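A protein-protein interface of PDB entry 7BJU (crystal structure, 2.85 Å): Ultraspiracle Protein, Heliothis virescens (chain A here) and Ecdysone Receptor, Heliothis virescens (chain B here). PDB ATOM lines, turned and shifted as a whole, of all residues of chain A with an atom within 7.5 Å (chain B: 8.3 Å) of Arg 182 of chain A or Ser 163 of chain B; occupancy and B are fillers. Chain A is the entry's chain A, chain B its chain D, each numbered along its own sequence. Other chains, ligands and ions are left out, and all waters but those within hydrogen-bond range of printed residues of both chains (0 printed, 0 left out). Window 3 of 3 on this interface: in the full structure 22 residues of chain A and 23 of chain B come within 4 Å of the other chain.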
ATOM      1  N   LEU A  70      10.490  15.475  27.222  1.00  0.00           N
ATOM      2  CA  LEU A  70       9.314  16.007  26.557  1.00  0.00           C
ATOM      3  C   LEU A  70       8.197  14.966  26.554  1.00  0.00           C
ATOM      4  O   LEU A  70       8.412  13.782  26.825  1.00  0.00           O
ATOM      5  CB  LEU A  70       9.641  16.418  25.121  1.00  0.00           C
ATOM      6  CG  LEU A  70      10.606  17.581  24.901  1.00  0.00           C
ATOM      7  CD1 LEU A  70      10.943  17.715  23.424  1.00  0.00           C
ATOM      8  CD2 LEU A  70      10.004  18.868  25.431  1.00  0.00           C
ATOM      9  N   ASP A  74       4.982  14.784  21.610  1.00  0.00           N
ATOM     10  CA  ASP A  74       5.791  15.878  21.082  1.00  0.00           C
ATOM     11  C   ASP A  74       7.085  15.360  20.470  1.00  0.00           C
ATOM     12  O   ASP A  74       7.546  15.879  19.447  1.00  0.00           O
ATOM     13  CB  ASP A  74       6.089  16.896  22.182  1.00  0.00           C
ATOM     14  CG  ASP A  74       4.910  17.798  22.475  1.00  0.00           C
ATOM     15  OD1 ASP A  74       3.886  17.677  21.772  1.00  0.00           O
ATOM     16  OD2 ASP A  74       5.008  18.626  23.404  1.00  0.00           O
ATOM     17  N   ASN A 173      11.953  22.430  16.836  1.00  0.00           N
ATOM     18  CA  ASN A 173      11.113  23.436  16.202  1.00  0.00           C
ATOM     19  C   ASN A 173       9.814  23.571  16.983  1.00  0.00           C
ATOM     20  O   ASN A 173       8.978  22.657  16.941  1.00  0.00           O
ATOM     21  CB  ASN A 173      10.828  23.061  14.750  1.00  0.00           C
ATOM     22  CG  ASN A 173       9.923  24.061  14.046  1.00  0.00           C
ATOM     23  OD1 ASN A 173       9.726  25.185  14.511  1.00  0.00           O
ATOM     24  ND2 ASN A 173       9.370  23.651  12.911  1.00  0.00           N
ATOM     25  N   PRO A 174       9.598  24.673  17.703  1.00  0.00           N
ATOM     26  CA  PRO A 174       8.344  24.849  18.445  1.00  0.00           C
ATOM     27  C   PRO A 174       7.149  25.199  17.575  1.00  0.00           C
ATOM     28  O   PRO A 174       6.033  25.286  18.099  1.00  0.00           O
ATOM     29  CB  PRO A 174       8.679  26.002  19.400  1.00  0.00           C
ATOM     30  CG  PRO A 174       9.699  26.802  18.663  1.00  0.00           C
ATOM     31  CD  PRO A 174      10.524  25.803  17.896  1.00  0.00           C
ATOM     32  N   ASP A 175       7.343  25.401  16.273  1.00  0.00           N
ATOM     33  CA  ASP A 175       6.258  25.750  15.367  1.00  0.00           C
ATOM     34  C   ASP A 175       5.619  24.534  14.710  1.00  0.00           C
ATOM     35  O   ASP A 175       4.764  24.698  13.832  1.00  0.00           O
ATOM     36  CB  ASP A 175       6.762  26.719  14.293  1.00  0.00           C
ATOM     37  CG  ASP A 175       7.125  28.078  14.859  1.00  0.00           C
ATOM     38  OD1 ASP A 175       6.503  28.487  15.861  1.00  0.00           O
ATOM     39  OD2 ASP A 175       8.033  28.736  14.305  1.00  0.00           O
ATOM     40  N   VAL A 176       6.009  23.324  15.111  1.00  0.00           N
ATOM     41  CA  VAL A 176       5.407  22.116  14.558  1.00  0.00           C
ATOM     42  C   VAL A 176       3.947  22.038  14.984  1.00  0.00           C
ATOM     43  O   VAL A 176       3.627  22.116  16.177  1.00  0.00           O
ATOM     44  CB  VAL A 176       6.186  20.872  15.007  1.00  0.00           C
ATOM     45  CG1 VAL A 176       5.413  19.605  14.672  1.00  0.00           C
ATOM     46  CG2 VAL A 176       7.564  20.846  14.363  1.00  0.00           C
ATOM     47  N   LEU A 179       1.801  20.036  18.549  1.00  0.00           N
ATOM     48  CA  LEU A 179       2.478  19.868  19.829  1.00  0.00           C
ATOM     49  C   LEU A 179       1.530  20.194  20.977  1.00  0.00           C
ATOM     50  O   LEU A 179       0.662  21.064  20.865  1.00  0.00           O
ATOM     51  CB  LEU A 179       3.711  20.770  19.904  1.00  0.00           C
ATOM     52  CG  LEU A 179       4.852  20.540  18.911  1.00  0.00           C
ATOM     53  CD1 LEU A 179       5.906  21.626  19.049  1.00  0.00           C
ATOM     54  CD2 LEU A 179       5.473  19.165  19.108  1.00  0.00           C
ATOM     55  N   LYS A 180       1.699  19.482  22.093  1.00  0.00           N
ATOM     56  CA  LYS A 180       0.918  19.691  23.307  1.00  0.00           C
ATOM     57  C   LYS A 180       1.622  20.571  24.329  1.00  0.00           C
ATOM     58  O   LYS A 180       0.971  21.076  25.250  1.00  0.00           O
ATOM     59  CB  LYS A 180       0.591  18.346  23.969  1.00  0.00           C
ATOM     60  CG  LYS A 180      -0.326  17.437  23.169  1.00  0.00           C
ATOM     61  CD  LYS A 180      -0.714  16.213  23.987  1.00  0.00           C
ATOM     62  CE  LYS A 180      -1.744  15.360  23.267  1.00  0.00           C
ATOM     63  NZ  LYS A 180      -2.179  14.204  24.100  1.00  0.00           N
ATOM     64  N   ASN A 181       2.947  20.739  24.208  1.00  0.00           N
ATOM     65  CA  ASN A 181       3.731  21.563  25.124  1.00  0.00           C
ATOM     66  C   ASN A 181       4.725  22.372  24.285  1.00  0.00           C
ATOM     67  O   ASN A 181       5.928  22.110  24.265  1.00  0.00           O
ATOM     68  CB  ASN A 181       4.435  20.716  26.186  1.00  0.00           C
ATOM     69  CG  ASN A 181       3.463  20.054  27.149  1.00  0.00           C
ATOM     70  OD1 ASN A 181       2.500  20.676  27.601  1.00  0.00           O
ATOM     71  ND2 ASN A 181       3.703  18.784  27.458  1.00  0.00           N
ATOM     72  N   ARG A 182       4.202  23.380  23.585  1.00  0.00           N
ATOM     73  CA  ARG A 182       5.033  24.195  22.704  1.00  0.00           C
ATOM     74  C   ARG A 182       6.146  24.894  23.474  1.00  0.00           C
ATOM     75  O   ARG A 182       7.284  24.975  22.996  1.00  0.00           O
ATOM     76  CB  ARG A 182       4.165  25.218  21.971  1.00  0.00           C
ATOM     77  CG  ARG A 182       4.943  26.230  21.145  1.00  0.00           C
ATOM     78  CD  ARG A 182       4.002  27.118  20.349  1.00  0.00           C
ATOM     79  NE  ARG A 182       4.713  27.927  19.367  1.00  0.00           N
ATOM     80  CZ  ARG A 182       5.062  29.193  19.552  1.00  0.00           C
ATOM     81  NH1 ARG A 182       4.774  29.833  20.674  1.00  0.00           N
ATOM     82  NH2 ARG A 182       5.714  29.834  18.586  1.00  0.00           N
ATOM     83  N   GLN A 183       5.840  25.401  24.669  1.00  0.00           N
ATOM     84  CA  GLN A 183       6.834  26.162  25.416  1.00  0.00           C
ATOM     85  C   GLN A 183       7.983  25.283  25.894  1.00  0.00           C
ATOM     86  O   GLN A 183       9.119  25.758  25.994  1.00  0.00           O
ATOM     87  CB  GLN A 183       6.172  26.879  26.591  1.00  0.00           C
ATOM     88  CG  GLN A 183       5.168  27.938  26.163  1.00  0.00           C
ATOM     89  CD  GLN A 183       5.263  29.205  26.992  1.00  0.00           C
ATOM     90  OE1 GLN A 183       5.714  29.180  28.137  1.00  0.00           O
ATOM     91  NE2 GLN A 183       4.844  30.325  26.412  1.00  0.00           N
ATOM     92  N   GLU A 184       7.719  24.004  26.185  1.00  0.00           N
ATOM     93  CA  GLU A 184       8.813  23.101  26.532  1.00  0.00           C
ATOM     94  C   GLU A 184       9.778  22.923  25.366  1.00  0.00           C
ATOM     95  O   GLU A 184      10.963  22.644  25.579  1.00  0.00           O
ATOM     96  CB  GLU A 184       8.267  21.743  26.977  1.00  0.00           C
ATOM     97  CG  GLU A 184       7.453  21.784  28.256  1.00  0.00           C
ATOM     98  CD  GLU A 184       7.124  20.399  28.782  1.00  0.00           C
ATOM     99  OE1 GLU A 184       7.993  19.504  28.695  1.00  0.00           O
ATOM    100  OE2 GLU A 184       5.996  20.203  29.282  1.00  0.00           O
ATOM    101  N   VAL A 185       9.293  23.079  24.134  1.00  0.00           N
ATOM    102  CA  VAL A 185      10.174  23.019  22.974  1.00  0.00           C
ATOM    103  C   VAL A 185      10.845  24.367  22.740  1.00  0.00           C
ATOM    104  O   VAL A 185      12.005  24.428  22.317  1.00  0.00           O
ATOM    105  CB  VAL A 185       9.390  22.552  21.735  1.00  0.00           C
ATOM    106  CG1 VAL A 185      10.324  22.372  20.548  1.00  0.00           C
ATOM    107  CG2 VAL A 185       8.646  21.262  22.036  1.00  0.00           C
ATOM    108  N   GLU A 186      10.128  25.463  23.004  1.00  0.00           N
ATOM    109  CA  GLU A 186      10.726  26.790  22.893  1.00  0.00           C
ATOM    110  C   GLU A 186      11.961  26.908  23.776  1.00  0.00           C
ATOM    111  O   GLU A 186      13.018  27.363  23.329  1.00  0.00           O
ATOM    112  CB  GLU A 186       9.712  27.871  23.272  1.00  0.00           C
ATOM    113  CG  GLU A 186       8.568  28.070  22.300  1.00  0.00           C
ATOM    114  CD  GLU A 186       7.860  29.391  22.522  1.00  0.00           C
ATOM    115  OE1 GLU A 186       8.452  30.442  22.199  1.00  0.00           O
ATOM    116  OE2 GLU A 186       6.721  29.382  23.035  1.00  0.00           O
ATOM    117  N   VAL A 187      11.840  26.493  25.040  1.00  0.00           N
ATOM    118  CA  VAL A 187      12.944  26.622  25.988  1.00  0.00           C
ATOM    119  C   VAL A 187      14.182  25.896  25.474  1.00  0.00           C
ATOM    120  O   VAL A 187      15.314  26.357  25.664  1.00  0.00           O
ATOM    121  CB  VAL A 187      12.510  26.107  27.375  1.00  0.00           C
ATOM    122  CG1 VAL A 187      13.657  26.184  28.359  1.00  0.00           C
ATOM    123  CG2 VAL A 187      11.326  26.909  27.897  1.00  0.00           C
ATOM    124  N   LEU A 188      13.987  24.767  24.789  1.00  0.00           N
ATOM    125  CA  LEU A 188      15.123  24.001  24.283  1.00  0.00           C
ATOM    126  C   LEU A 188      15.781  24.698  23.096  1.00  0.00           C
ATOM    127  O   LEU A 188      17.011  24.822  23.045  1.00  0.00           O
ATOM    128  CB  LEU A 188      14.675  22.590  23.905  1.00  0.00           C
ATOM    129  CG  LEU A 188      14.223  21.712  25.073  1.00  0.00           C
ATOM    130  CD1 LEU A 188      13.806  20.338  24.581  1.00  0.00           C
ATOM    131  CD2 LEU A 188      15.325  21.599  26.118  1.00  0.00           C
ATOM    132  N   ALA B 119      -0.656  37.803   8.709  1.00  0.00           N
ATOM    133  CA  ALA B 119      -0.394  37.411  10.091  1.00  0.00           C
ATOM    134  C   ALA B 119      -0.300  38.620  11.011  1.00  0.00           C
ATOM    135  O   ALA B 119      -0.674  38.535  12.187  1.00  0.00           O
ATOM    136  CB  ALA B 119       0.889  36.583  10.171  1.00  0.00           C
ATOM    137  N   TYR B 122      -3.547  39.597  12.969  1.00  0.00           N
ATOM    138  CA  TYR B 122      -4.201  38.585  13.783  1.00  0.00           C
ATOM    139  C   TYR B 122      -4.701  39.199  15.084  1.00  0.00           C
ATOM    140  O   TYR B 122      -3.982  39.956  15.742  1.00  0.00           O
ATOM    141  CB  TYR B 122      -3.238  37.430  14.073  1.00  0.00           C
ATOM    142  CG  TYR B 122      -3.724  36.470  15.138  1.00  0.00           C
ATOM    143  CD1 TYR B 122      -4.645  35.475  14.836  1.00  0.00           C
ATOM    144  CD2 TYR B 122      -3.255  36.553  16.443  1.00  0.00           C
ATOM    145  CE1 TYR B 122      -5.090  34.596  15.805  1.00  0.00           C
ATOM    146  CE2 TYR B 122      -3.695  35.678  17.419  1.00  0.00           C
ATOM    147  CZ  TYR B 122      -4.612  34.703  17.094  1.00  0.00           C
ATOM    148  OH  TYR B 122      -5.050  33.830  18.062  1.00  0.00           O
ATOM    149  N   ALA B 124      -6.048  38.193  18.788  1.00  0.00           N
ATOM    150  CA  ALA B 124      -6.060  37.047  19.691  1.00  0.00           C
ATOM    151  C   ALA B 124      -7.440  36.826  20.299  1.00  0.00           C
ATOM    152  O   ALA B 124      -7.853  35.679  20.509  1.00  0.00           O
ATOM    153  CB  ALA B 124      -5.015  37.236  20.789  1.00  0.00           C
ATOM    154  N   HIS B 156      -2.558  29.002  12.356  1.00  0.00           N
ATOM    155  CA  HIS B 156      -1.475  28.490  13.192  1.00  0.00           C
ATOM    156  C   HIS B 156      -0.241  29.374  13.077  1.00  0.00           C
ATOM    157  O   HIS B 156       0.384  29.725  14.084  1.00  0.00           O
ATOM    158  CB  HIS B 156      -1.142  27.049  12.803  1.00  0.00           C
ATOM    159  CG  HIS B 156       0.047  26.490  13.522  1.00  0.00           C
ATOM    160  ND1 HIS B 156       0.070  26.299  14.887  1.00  0.00           N
ATOM    161  CD2 HIS B 156       1.255  26.083  13.065  1.00  0.00           C
ATOM    162  CE1 HIS B 156       1.240  25.796  15.241  1.00  0.00           C
ATOM    163  NE2 HIS B 156       1.976  25.654  14.154  1.00  0.00           N
ATOM    164  N   PHE B 157       0.125  29.744  11.846  1.00  0.00           N
ATOM    165  CA  PHE B 157       1.229  30.676  11.654  1.00  0.00           C
ATOM    166  C   PHE B 157       0.921  32.025  12.292  1.00  0.00           C
ATOM    167  O   PHE B 157       1.803  32.658  12.886  1.00  0.00           O
ATOM    168  CB  PHE B 157       1.523  30.838  10.163  1.00  0.00           C
ATOM    169  CG  PHE B 157       2.629  31.808   9.863  1.00  0.00           C
ATOM    170  CD1 PHE B 157       3.955  31.432  10.012  1.00  0.00           C
ATOM    171  CD2 PHE B 157       2.346  33.092   9.429  1.00  0.00           C
ATOM    172  CE1 PHE B 157       4.977  32.320   9.736  1.00  0.00           C
ATOM    173  CE2 PHE B 157       3.364  33.984   9.155  1.00  0.00           C
ATOM    174  CZ  PHE B 157       4.681  33.598   9.309  1.00  0.00           C
ATOM    175  N   CYS B 158      -0.330  32.477  12.182  1.00  0.00           N
ATOM    176  CA  CYS B 158      -0.728  33.734  12.808  1.00  0.00           C
ATOM    177  C   CYS B 158      -0.523  33.682  14.317  1.00  0.00           C
ATOM    178  O   CYS B 158       0.021  34.617  14.915  1.00  0.00           O
ATOM    179  CB  CYS B 158      -2.187  34.047  12.470  1.00  0.00           C
ATOM    180  SG  CYS B 158      -2.483  34.493  10.744  1.00  0.00           S
ATOM    181  N   ARG B 159      -0.952  32.586  14.950  1.00  0.00           N
ATOM    182  CA  ARG B 159      -0.738  32.432  16.387  1.00  0.00           C
ATOM    183  C   ARG B 159       0.746  32.367  16.720  1.00  0.00           C
ATOM    184  O   ARG B 159       1.199  32.982  17.693  1.00  0.00           O
ATOM    185  CB  ARG B 159      -1.451  31.179  16.897  1.00  0.00           C
ATOM    186  CG  ARG B 159      -2.946  31.147  16.628  1.00  0.00           C
ATOM    187  CD  ARG B 159      -3.560  29.840  17.103  1.00  0.00           C
ATOM    188  NE  ARG B 159      -4.961  29.719  16.720  1.00  0.00           N
ATOM    189  CZ  ARG B 159      -5.403  28.985  15.708  1.00  0.00           C
ATOM    190  NH1 ARG B 159      -4.577  28.278  14.954  1.00  0.00           N
ATOM    191  NH2 ARG B 159      -6.707  28.955  15.448  1.00  0.00           N
ATOM    192  N   CYS B 160       1.521  31.626  15.923  1.00  0.00           N
ATOM    193  CA  CYS B 160       2.948  31.489  16.199  1.00  0.00           C
ATOM    194  C   CYS B 160       3.673  32.821  16.059  1.00  0.00           C
ATOM    195  O   CYS B 160       4.557  33.142  16.861  1.00  0.00           O
ATOM    196  CB  CYS B 160       3.566  30.440  15.274  1.00  0.00           C
ATOM    197  SG  CYS B 160       3.152  28.731  15.697  1.00  0.00           S
ATOM    198  N   MET B 161       3.315  33.613  15.046  1.00  0.00           N
ATOM    199  CA  MET B 161       3.975  34.901  14.860  1.00  0.00           C
ATOM    200  C   MET B 161       3.510  35.915  15.898  1.00  0.00           C
ATOM    201  O   MET B 161       4.303  36.742  16.364  1.00  0.00           O
ATOM    202  CB  MET B 161       3.723  35.425  13.447  1.00  0.00           C
ATOM    203  CG  MET B 161       4.976  35.941  12.757  1.00  0.00           C
ATOM    204  SD  MET B 161       4.609  36.870  11.259  1.00  0.00           S
ATOM    205  CE  MET B 161       3.651  38.220  11.939  1.00  0.00           C
ATOM    206  N   TYR B 162       2.227  35.866  16.272  1.00  0.00           N
ATOM    207  CA  TYR B 162       1.699  36.809  17.254  1.00  0.00           C
ATOM    208  C   TYR B 162       2.391  36.647  18.601  1.00  0.00           C
ATOM    209  O   TYR B 162       2.620  37.632  19.313  1.00  0.00           O
ATOM    210  CB  TYR B 162       0.189  36.618  17.398  1.00  0.00           C
ATOM    211  CG  TYR B 162      -0.459  37.484  18.455  1.00  0.00           C
ATOM    212  CD1 TYR B 162      -0.806  38.801  18.185  1.00  0.00           C
ATOM    213  CD2 TYR B 162      -0.738  36.980  19.718  1.00  0.00           C
ATOM    214  CE1 TYR B 162      -1.404  39.594  19.148  1.00  0.00           C
ATOM    215  CE2 TYR B 162      -1.335  37.765  20.686  1.00  0.00           C
ATOM    216  CZ  TYR B 162      -1.665  39.071  20.397  1.00  0.00           C
ATOM    217  OH  TYR B 162      -2.262  39.853  21.361  1.00  0.00           O
ATOM    218  N   SER B 163       2.736  35.411  18.965  1.00  0.00           N
ATOM    219  CA  SER B 163       3.383  35.150  20.244  1.00  0.00           C
ATOM    220  C   SER B 163       4.811  35.674  20.302  1.00  0.00           C
ATOM    221  O   SER B 163       5.375  35.760  21.399  1.00  0.00           O
ATOM    222  CB  SER B 163       3.371  33.648  20.539  1.00  0.00           C
ATOM    223  OG  SER B 163       4.133  32.933  19.583  1.00  0.00           O
ATOM    224  N   MET B 164       5.407  36.030  19.163  1.00  0.00           N
ATOM    225  CA  MET B 164       6.754  36.587  19.165  1.00  0.00           C
ATOM    226  C   MET B 164       6.790  38.036  19.632  1.00  0.00           C
ATOM    227  O   MET B 164       7.840  38.491  20.101  1.00  0.00           O
ATOM    228  CB  MET B 164       7.372  36.480  17.771  1.00  0.00           C
ATOM    229  CG  MET B 164       7.652  35.055  17.332  1.00  0.00           C
ATOM    230  SD  MET B 164       8.824  35.003  15.971  1.00  0.00           S
ATOM    231  CE  MET B 164      10.084  36.112  16.595  1.00  0.00           C
ATOM    232  N   MET B 165       5.677  38.761  19.515  1.00  0.00           N
ATOM    233  CA  MET B 165       5.566  40.149  19.963  1.00  0.00           C
ATOM    234  C   MET B 165       6.592  41.038  19.257  1.00  0.00           C
ATOM    235  O   MET B 165       7.399  41.728  19.883  1.00  0.00           O
ATOM    236  CB  MET B 165       5.702  40.244  21.487  1.00  0.00           C
ATOM    237  CG  MET B 165       4.639  39.473  22.247  1.00  0.00           C
ATOM    238  SD  MET B 165       2.988  40.139  21.969  1.00  0.00           S
ATOM    239  CE  MET B 165       1.979  38.874  22.733  1.00  0.00           C
ATOM    240  N   MET B 166       6.545  41.011  17.928  1.00  0.00           N
ATOM    241  CA  MET B 166       7.406  41.865  17.124  1.00  0.00           C
ATOM    242  C   MET B 166       6.838  43.277  17.077  1.00  0.00           C
ATOM    243  O   MET B 166       5.637  43.465  16.855  1.00  0.00           O
ATOM    244  CB  MET B 166       7.545  41.317  15.702  1.00  0.00           C
ATOM    245  CG  MET B 166       8.153  39.928  15.599  1.00  0.00           C
ATOM    246  SD  MET B 166       8.230  39.325  13.897  1.00  0.00           S
ATOM    247  CE  MET B 166       9.656  40.204  13.264  1.00  0.00           C
ATOM    248  N   LYS B 223      14.875  33.793  16.735  1.00  0.00           N
ATOM    249  CA  LYS B 223      13.472  33.477  16.486  1.00  0.00           C
ATOM    250  C   LYS B 223      12.941  34.229  15.272  1.00  0.00           C
ATOM    251  O   LYS B 223      12.150  33.678  14.494  1.00  0.00           O
ATOM    252  CB  LYS B 223      12.631  33.791  17.725  1.00  0.00           C
ATOM    253  CG  LYS B 223      12.894  32.863  18.900  1.00  0.00           C
ATOM    254  CD  LYS B 223      11.684  32.742  19.815  1.00  0.00           C
ATOM    255  CE  LYS B 223      11.365  34.047  20.519  1.00  0.00           C
ATOM    256  NZ  LYS B 223      10.221  33.891  21.464  1.00  0.00           N
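The side-chain carboxylate of Asp 175 of chain A sits at hydrogen-bond distance from the side-chain sulfur of Cys 160 of chain B. The backbone carbonyl oxygen (O) of Asp 175 of chain A sits at hydrogen-bond distance from a ring nitrogen (NE2) of His 156 of chain B, at 3.0 Å. The side-chain carboxylate (OE1) of Glu 186 of chain A is in salt-bridge range of the side-chain amino group (NZ) of Lys 223 of chain B (3.9 Å). OG of Ser 163 of chain B sits at hydrogen-bond distance from NH1 of Arg 182 of chain A.
Along chain B the printed residues that touch a printed residue of chain A span positions 156 to 223. Among the printed residues, Asp or Glu carboxylates within 4 Å of a Lys or Arg side-chain nitrogen of the other chain: Glu 186 of chain A with Lys 223 of chain B (3.9 Å).
Among the printed residues, merely in contact across the chains: Arg 182 of chain A with Cys 160 of chain B (3.9 Å).
Of chain B, only Cys 160 (3.9 Å) and Ser 163 (3.3 Å) come within 4 Å of Arg 182 of chain A. Ser 163 of chain B touches one residue of chain A. Printed residues of chain A within 4 Å of Cys 160 of chain B: Asp 175 (3.4 Å) and Arg 182 (3.9 Å). Printed residues of chain A within 4 Å of His 156 of chain B: Asp 175. Printed residues of chain B within 4 Å of Glu 186 of chain A: Lys 223 (3.9 Å). Of the printed residues of chain B, Asp 175 of chain A touches His 156 (3.0 Å) and Cys 160 (3.4 Å). Printed residues of chain A within 4 Å of Lys 223 of chain B: Glu 186. Met 161 of chain B touches none of the printed residues of chain A.
The side-chain carboxylate of Glu 186 of chain A lies within salt-bridge range of the guanidinium group of Arg 182 of chain A, at 3.1 Å. OG of Ser 163 of chain B is in hydrogen-bond range of O of Cys 160 of chain B (2.8 Å). The side-chain hydroxyl (OG) of Ser 163 of chain B sits at hydrogen-bond distance from the backbone carbonyl oxygen (O) of Arg 159 of chain B. O of Pro 174 of chain A lies within hydrogen-bond range of NE of Arg 182 of chain A (3.2 Å). The side-chain amide oxygen (OD1) of Asn 173 of chain A lies within hydrogen-bond range of the backbone NH (N) of Asp 175 of chain A, 3.0 Å away. The side-chain sulfur (SG) of Cys 160 of chain B sits at hydrogen-bond distance from the backbone carbonyl oxygen (O) of His 156 of chain B (3.4 Å).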
